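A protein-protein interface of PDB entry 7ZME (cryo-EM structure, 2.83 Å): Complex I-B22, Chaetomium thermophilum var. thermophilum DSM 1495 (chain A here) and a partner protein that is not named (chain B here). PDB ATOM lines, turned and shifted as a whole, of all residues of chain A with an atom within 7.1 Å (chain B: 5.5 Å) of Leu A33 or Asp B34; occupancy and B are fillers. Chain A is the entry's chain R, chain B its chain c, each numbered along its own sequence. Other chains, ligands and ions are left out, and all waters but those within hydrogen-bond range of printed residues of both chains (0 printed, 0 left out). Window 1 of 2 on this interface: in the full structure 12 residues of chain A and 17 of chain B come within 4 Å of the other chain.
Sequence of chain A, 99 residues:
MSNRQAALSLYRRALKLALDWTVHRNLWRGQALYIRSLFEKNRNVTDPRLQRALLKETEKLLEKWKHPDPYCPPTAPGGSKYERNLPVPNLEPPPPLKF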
ATOM      1  N   TYR A  11      10.638   1.487   0.092  1.00  0.00           N
ATOM      2  CA  TYR A  11      10.095   2.690   0.780  1.00  0.00           C
ATOM      3  C   TYR A  11       8.967   2.263   1.716  1.00  0.00           C
ATOM      4  O   TYR A  11       8.988   2.644   2.893  1.00  0.00           O
ATOM      5  CB  TYR A  11       9.581   3.718  -0.225  1.00  0.00           C
ATOM      6  CG  TYR A  11       9.071   5.007   0.367  1.00  0.00           C
ATOM      7  CD1 TYR A  11       9.888   5.818   1.131  1.00  0.00           C
ATOM      8  CD2 TYR A  11       7.774   5.431   0.140  1.00  0.00           C
ATOM      9  CE1 TYR A  11       9.432   7.011   1.664  1.00  0.00           C
ATOM     10  CE2 TYR A  11       7.301   6.623   0.659  1.00  0.00           C
ATOM     11  CZ  TYR A  11       8.134   7.416   1.425  1.00  0.00           C
ATOM     12  OH  TYR A  11       7.672   8.587   1.947  1.00  0.00           O
ATOM     13  N   LEU A  15       8.823   2.414   5.910  1.00  0.00           N
ATOM     14  CA  LEU A  15       7.795   3.125   6.708  1.00  0.00           C
ATOM     15  C   LEU A  15       7.079   2.093   7.559  1.00  0.00           C
ATOM     16  O   LEU A  15       6.780   2.390   8.717  1.00  0.00           O
ATOM     17  CB  LEU A  15       6.815   3.810   5.761  1.00  0.00           C
ATOM     18  CG  LEU A  15       7.439   4.768   4.747  1.00  0.00           C
ATOM     19  CD1 LEU A  15       6.365   5.414   3.890  1.00  0.00           C
ATOM     20  CD2 LEU A  15       8.272   5.831   5.441  1.00  0.00           C
ATOM     21  N   TRP A  28       6.174   8.053  14.659  1.00  0.00           N
ATOM     22  CA  TRP A  28       6.504   7.494  13.355  1.00  0.00           C
ATOM     23  C   TRP A  28       6.341   8.528  12.253  1.00  0.00           C
ATOM     24  O   TRP A  28       7.040   8.465  11.236  1.00  0.00           O
ATOM     25  CB  TRP A  28       5.626   6.272  13.085  1.00  0.00           C
ATOM     26  CG  TRP A  28       5.573   5.845  11.659  1.00  0.00           C
ATOM     27  CD1 TRP A  28       6.552   5.220  10.959  1.00  0.00           C
ATOM     28  CD2 TRP A  28       4.471   5.999  10.759  1.00  0.00           C
ATOM     29  NE1 TRP A  28       6.136   4.976   9.675  1.00  0.00           N
ATOM     30  CE2 TRP A  28       4.860   5.446   9.527  1.00  0.00           C
ATOM     31  CE3 TRP A  28       3.196   6.555  10.876  1.00  0.00           C
ATOM     32  CZ2 TRP A  28       4.023   5.431   8.420  1.00  0.00           C
ATOM     33  CZ3 TRP A  28       2.366   6.539   9.777  1.00  0.00           C
ATOM     34  CH2 TRP A  28       2.781   5.980   8.565  1.00  0.00           C
ATOM     35  N   ARG A  29       5.433   9.486  12.441  1.00  0.00           N
ATOM     36  CA  ARG A  29       5.246  10.533  11.444  1.00  0.00           C
ATOM     37  C   ARG A  29       6.519  11.344  11.262  1.00  0.00           C
ATOM     38  O   ARG A  29       6.898  11.675  10.132  1.00  0.00           O
ATOM     39  CB  ARG A  29       4.081  11.433  11.845  1.00  0.00           C
ATOM     40  CG  ARG A  29       3.600  12.337  10.734  1.00  0.00           C
ATOM     41  CD  ARG A  29       2.747  11.573   9.739  1.00  0.00           C
ATOM     42  NE  ARG A  29       3.429  11.397   8.461  1.00  0.00           N
ATOM     43  CZ  ARG A  29       2.888  10.806   7.402  1.00  0.00           C
ATOM     44  NH1 ARG A  29       1.652  10.331   7.466  1.00  0.00           N
ATOM     45  NH2 ARG A  29       3.581  10.687   6.278  1.00  0.00           N
ATOM     46  N   GLY A  30       7.195  11.673  12.361  1.00  0.00           N
ATOM     47  CA  GLY A  30       8.503  12.295  12.244  1.00  0.00           C
ATOM     48  C   GLY A  30       9.513  11.380  11.581  1.00  0.00           C
ATOM     49  O   GLY A  30      10.320  11.819  10.760  1.00  0.00           O
ATOM     50  N   GLN A  31       9.485  10.096  11.938  1.00  0.00           N
ATOM     51  CA  GLN A  31      10.391   9.130  11.328  1.00  0.00           C
ATOM     52  C   GLN A  31      10.101   8.967   9.843  1.00  0.00           C
ATOM     53  O   GLN A  31      11.024   8.911   9.024  1.00  0.00           O
ATOM     54  CB  GLN A  31      10.260   7.782  12.029  1.00  0.00           C
ATOM     55  CG  GLN A  31      11.020   7.666  13.325  1.00  0.00           C
ATOM     56  CD  GLN A  31      10.344   6.720  14.286  1.00  0.00           C
ATOM     57  OE1 GLN A  31       9.769   5.714  13.875  1.00  0.00           O
ATOM     58  NE2 GLN A  31      10.410   7.031  15.571  1.00  0.00           N
ATOM     59  N   ALA A  32       8.819   8.872   9.482  1.00  0.00           N
ATOM     60  CA  ALA A  32       8.450   8.688   8.083  1.00  0.00           C
ATOM     61  C   ALA A  32       8.873   9.884   7.243  1.00  0.00           C
ATOM     62  O   ALA A  32       9.323   9.725   6.102  1.00  0.00           O
ATOM     63  CB  ALA A  32       6.948   8.450   7.965  1.00  0.00           C
ATOM     64  N   LEU A  33       8.730  11.093   7.789  1.00  0.00           N
ATOM     65  CA  LEU A  33       9.180  12.281   7.075  1.00  0.00           C
ATOM     66  C   LEU A  33      10.688  12.265   6.866  1.00  0.00           C
ATOM     67  O   LEU A  33      11.175  12.747   5.838  1.00  0.00           O
ATOM     68  CB  LEU A  33       8.756  13.537   7.835  1.00  0.00           C
ATOM     69  CG  LEU A  33       9.098  14.873   7.179  1.00  0.00           C
ATOM     70  CD1 LEU A  33       8.379  15.006   5.847  1.00  0.00           C
ATOM     71  CD2 LEU A  33       8.743  16.027   8.101  1.00  0.00           C
ATOM     72  N   TYR A  34      11.437  11.716   7.824  1.00  0.00           N
ATOM     73  CA  TYR A  34      12.883  11.622   7.668  1.00  0.00           C
ATOM     74  C   TYR A  34      13.256  10.625   6.580  1.00  0.00           C
ATOM     75  O   TYR A  34      14.243  10.823   5.863  1.00  0.00           O
ATOM     76  CB  TYR A  34      13.528  11.229   8.995  1.00  0.00           C
ATOM     77  CG  TYR A  34      14.957  10.761   8.866  1.00  0.00           C
ATOM     78  CD1 TYR A  34      15.948  11.616   8.398  1.00  0.00           C
ATOM     79  CD2 TYR A  34      15.317   9.467   9.204  1.00  0.00           C
ATOM     80  CE1 TYR A  34      17.256  11.196   8.278  1.00  0.00           C
ATOM     81  CE2 TYR A  34      16.625   9.037   9.087  1.00  0.00           C
ATOM     82  CZ  TYR A  34      17.590   9.906   8.622  1.00  0.00           C
ATOM     83  OH  TYR A  34      18.893   9.481   8.503  1.00  0.00           O
ATOM     84  N   ILE A  35      12.486   9.544   6.448  1.00  0.00           N
ATOM     85  CA  ILE A  35      12.781   8.542   5.428  1.00  0.00           C
ATOM     86  C   ILE A  35      12.585   9.124   4.035  1.00  0.00           C
ATOM     87  O   ILE A  35      13.416   8.927   3.143  1.00  0.00           O
ATOM     88  CB  ILE A  35      11.921   7.285   5.645  1.00  0.00           C
ATOM     89  CG1 ILE A  35      12.188   6.693   7.027  1.00  0.00           C
ATOM     90  CG2 ILE A  35      12.195   6.257   4.561  1.00  0.00           C
ATOM     91  CD1 ILE A  35      13.623   6.259   7.233  1.00  0.00           C
ATOM     92  N   ARG A  36      11.484   9.852   3.828  1.00  0.00           N
ATOM     93  CA  ARG A  36      11.211  10.429   2.516  1.00  0.00           C
ATOM     94  C   ARG A  36      12.338  11.347   2.061  1.00  0.00           C
ATOM     95  O   ARG A  36      12.599  11.462   0.858  1.00  0.00           O
ATOM     96  CB  ARG A  36       9.884  11.188   2.543  1.00  0.00           C
ATOM     97  CG  ARG A  36       9.525  11.856   1.227  1.00  0.00           C
ATOM     98  CD  ARG A  36       8.231  12.644   1.327  1.00  0.00           C
ATOM     99  NE  ARG A  36       8.095  13.601   0.234  1.00  0.00           N
ATOM    100  CZ  ARG A  36       7.695  13.283  -0.993  1.00  0.00           C
ATOM    101  NH1 ARG A  36       7.599  14.218  -1.927  1.00  0.00           N
ATOM    102  NH2 ARG A  36       7.391  12.026  -1.287  1.00  0.00           N
ATOM    103  N   SER A  37      13.018  12.004   3.002  1.00  0.00           N
ATOM    104  CA  SER A  37      14.171  12.821   2.643  1.00  0.00           C
ATOM    105  C   SER A  37      15.288  11.968   2.057  1.00  0.00           C
ATOM    106  O   SER A  37      15.953  12.379   1.099  1.00  0.00           O
ATOM    107  CB  SER A  37      14.667  13.589   3.867  1.00  0.00           C
ATOM    108  OG  SER A  37      15.127  12.700   4.869  1.00  0.00           O
ATOM    109  N   LEU A  38      15.515  10.782   2.627  1.00  0.00           N
ATOM    110  CA  LEU A  38      16.578   9.914   2.133  1.00  0.00           C
ATOM    111  C   LEU A  38      16.296   9.447   0.712  1.00  0.00           C
ATOM    112  O   LEU A  38      17.203   9.402  -0.127  1.00  0.00           O
ATOM    113  CB  LEU A  38      16.750   8.718   3.066  1.00  0.00           C
ATOM    114  CG  LEU A  38      17.236   9.089   4.465  1.00  0.00           C
ATOM    115  CD1 LEU A  38      17.282   7.868   5.371  1.00  0.00           C
ATOM    116  CD2 LEU A  38      18.589   9.763   4.381  1.00  0.00           C
ATOM    117  N   PRO B  31       6.429  16.333  13.942  1.00  0.00           N
ATOM    118  CA  PRO B  31       7.053  17.314  13.047  1.00  0.00           C
ATOM    119  C   PRO B  31       6.289  18.628  13.041  1.00  0.00           C
ATOM    120  O   PRO B  31       5.067  18.660  13.200  1.00  0.00           O
ATOM    121  CB  PRO B  31       7.012  16.633  11.673  1.00  0.00           C
ATOM    122  CG  PRO B  31       6.082  15.461  11.806  1.00  0.00           C
ATOM    123  CD  PRO B  31       5.614  15.342  13.221  1.00  0.00           C
ATOM    124  N   THR B  32       7.034  19.723  12.863  1.00  0.00           N
ATOM    125  CA  THR B  32       6.405  21.036  12.782  1.00  0.00           C
ATOM    126  C   THR B  32       5.479  21.124  11.578  1.00  0.00           C
ATOM    127  O   THR B  32       4.369  21.660  11.675  1.00  0.00           O
ATOM    128  CB  THR B  32       7.472  22.128  12.717  1.00  0.00           C
ATOM    129  OG1 THR B  32       8.271  21.948  11.540  1.00  0.00           O
ATOM    130  CG2 THR B  32       8.367  22.071  13.944  1.00  0.00           C
ATOM    131  N   TYR B  33       5.916  20.605  10.434  1.00  0.00           N
ATOM    132  CA  TYR B  33       5.084  20.516   9.246  1.00  0.00           C
ATOM    133  C   TYR B  33       5.207  19.126   8.641  1.00  0.00           C
ATOM    134  O   TYR B  33       6.306  18.568   8.560  1.00  0.00           O
ATOM    135  CB  TYR B  33       5.466  21.563   8.198  1.00  0.00           C
ATOM    136  CG  TYR B  33       4.901  21.258   6.831  1.00  0.00           C
ATOM    137  CD1 TYR B  33       3.540  21.369   6.583  1.00  0.00           C
ATOM    138  CD2 TYR B  33       5.724  20.844   5.794  1.00  0.00           C
ATOM    139  CE1 TYR B  33       3.017  21.084   5.338  1.00  0.00           C
ATOM    140  CE2 TYR B  33       5.209  20.557   4.546  1.00  0.00           C
ATOM    141  CZ  TYR B  33       3.855  20.679   4.323  1.00  0.00           C
ATOM    142  OH  TYR B  33       3.336  20.395   3.081  1.00  0.00           O
ATOM    143  N   ASP B  34       4.075  18.578   8.220  1.00  0.00           N
ATOM    144  CA  ASP B  34       4.021  17.295   7.540  1.00  0.00           C
ATOM    145  C   ASP B  34       2.969  17.399   6.449  1.00  0.00           C
ATOM    146  O   ASP B  34       2.096  18.270   6.508  1.00  0.00           O
ATOM    147  CB  ASP B  34       3.688  16.158   8.516  1.00  0.00           C
ATOM    148  CG  ASP B  34       4.014  14.789   7.958  1.00  0.00           C
ATOM    149  OD1 ASP B  34       5.209  14.426   7.930  1.00  0.00           O
ATOM    150  OD2 ASP B  34       3.077  14.073   7.547  1.00  0.00           O
ATOM    151  N   PRO B  35       3.050  16.574   5.422  1.00  0.00           N
ATOM    152  CA  PRO B  35       1.990  16.586   4.407  1.00  0.00           C
ATOM    153  C   PRO B  35       0.722  15.875   4.848  1.00  0.00           C
ATOM    154  O   PRO B  35      -0.105  15.539   3.999  1.00  0.00           O
ATOM    155  CB  PRO B  35       2.635  15.860   3.220  1.00  0.00           C
ATOM    156  CG  PRO B  35       4.100  16.045   3.417  1.00  0.00           C
ATOM    157  CD  PRO B  35       4.302  15.998   4.901  1.00  0.00           C
ATOM    158  N   TRP B  36       0.548  15.615   6.151  1.00  0.00           N
ATOM    159  CA  TRP B  36      -0.494  14.672   6.539  1.00  0.00           C
ATOM    160  C   TRP B  36      -1.255  15.022   7.822  1.00  0.00           C
ATOM    161  O   TRP B  36      -1.981  14.162   8.335  1.00  0.00           O
ATOM    162  CB  TRP B  36       0.113  13.275   6.693  1.00  0.00           C
ATOM    163  CG  TRP B  36       0.069  12.421   5.457  1.00  0.00           C
ATOM    164  CD1 TRP B  36       1.134  11.919   4.776  1.00  0.00           C
ATOM    165  CD2 TRP B  36      -1.098  11.941   4.780  1.00  0.00           C
ATOM    166  NE1 TRP B  36       0.708  11.167   3.713  1.00  0.00           N
ATOM    167  CE2 TRP B  36      -0.660  11.166   3.694  1.00  0.00           C
ATOM    168  CE3 TRP B  36      -2.469  12.098   4.985  1.00  0.00           C
ATOM    169  CZ2 TRP B  36      -1.541  10.545   2.819  1.00  0.00           C
ATOM    170  CZ3 TRP B  36      -3.342  11.486   4.113  1.00  0.00           C
ATOM    171  CH2 TRP B  36      -2.876  10.721   3.040  1.00  0.00           C
ATOM    172  N   GLU B  37      -1.124  16.235   8.373  1.00  0.00           N
ATOM    173  CA  GLU B  37      -1.852  16.537   9.607  1.00  0.00           C
ATOM    174  C   GLU B  37      -3.357  16.481   9.393  1.00  0.00           C
ATOM    175  O   GLU B  37      -4.093  15.936  10.224  1.00  0.00           O
ATOM    176  CB  GLU B  37      -1.474  17.908  10.176  1.00  0.00           C
ATOM    177  CG  GLU B  37      -0.061  18.057  10.693  1.00  0.00           C
ATOM    178  CD  GLU B  37       0.909  18.354   9.592  1.00  0.00           C
ATOM    179  OE1 GLU B  37       0.448  18.500   8.446  1.00  0.00           O
ATOM    180  OE2 GLU B  37       2.120  18.471   9.876  1.00  0.00           O
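The guanidinium group of Arg A29 lies within salt-bridge range of the side-chain carboxylate of Asp B34 (2.8 Å).
The side-chain carboxylate (OE2) of Glu B37 sits at hydrogen-bond distance from the backbone NH (N) of Asp B34.
OD2 of Asp B34 sits close to N of Trp B36 (3.3 Å).
Arg A29 touches Trp B36 (NH2 to CD1, 3.1 Å).
Gly A30 touches Pro B31 (N to CG, 3.99 Å).
CD2 of Leu A33 touches O of Tyr B33, 3.6 Å away.
Leu A33 touches Asp B34.
Of the printed residues of chain B, Leu A33 touches Tyr B33 (3.6 Å) and Asp B34 (3.7 Å).
Arg A36 touches none of the printed residues of chain B.
Of the printed residues of chain A, Pro B31 touches Gly A30 (3.99 Å).
Printed residues of chain A within 4 Å of Tyr B33: Leu A33 (3.6 Å).
Of chain A, only Arg A29 and Leu A33 come within 4 Å of Asp B34.
Printed residues of chain A within 4 Å of Trp B36: Arg A29.
The nearest printed residue of chain B that does not touch Leu A33 is Pro B31 (4.02 Å).
Of the 7 printed residues of chain B, 4 touch a printed residue of chain A.
Hydrophobic or aromatic side chains of chain B within 4 Å of the printed part of chain A: Pro B31 and Trp B36.
Printed residues of chain A that touch a printed residue of chain B: Arg A29, Gly A30 and Leu A33.
Among the printed residues, 5 pairs touch across the chains.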
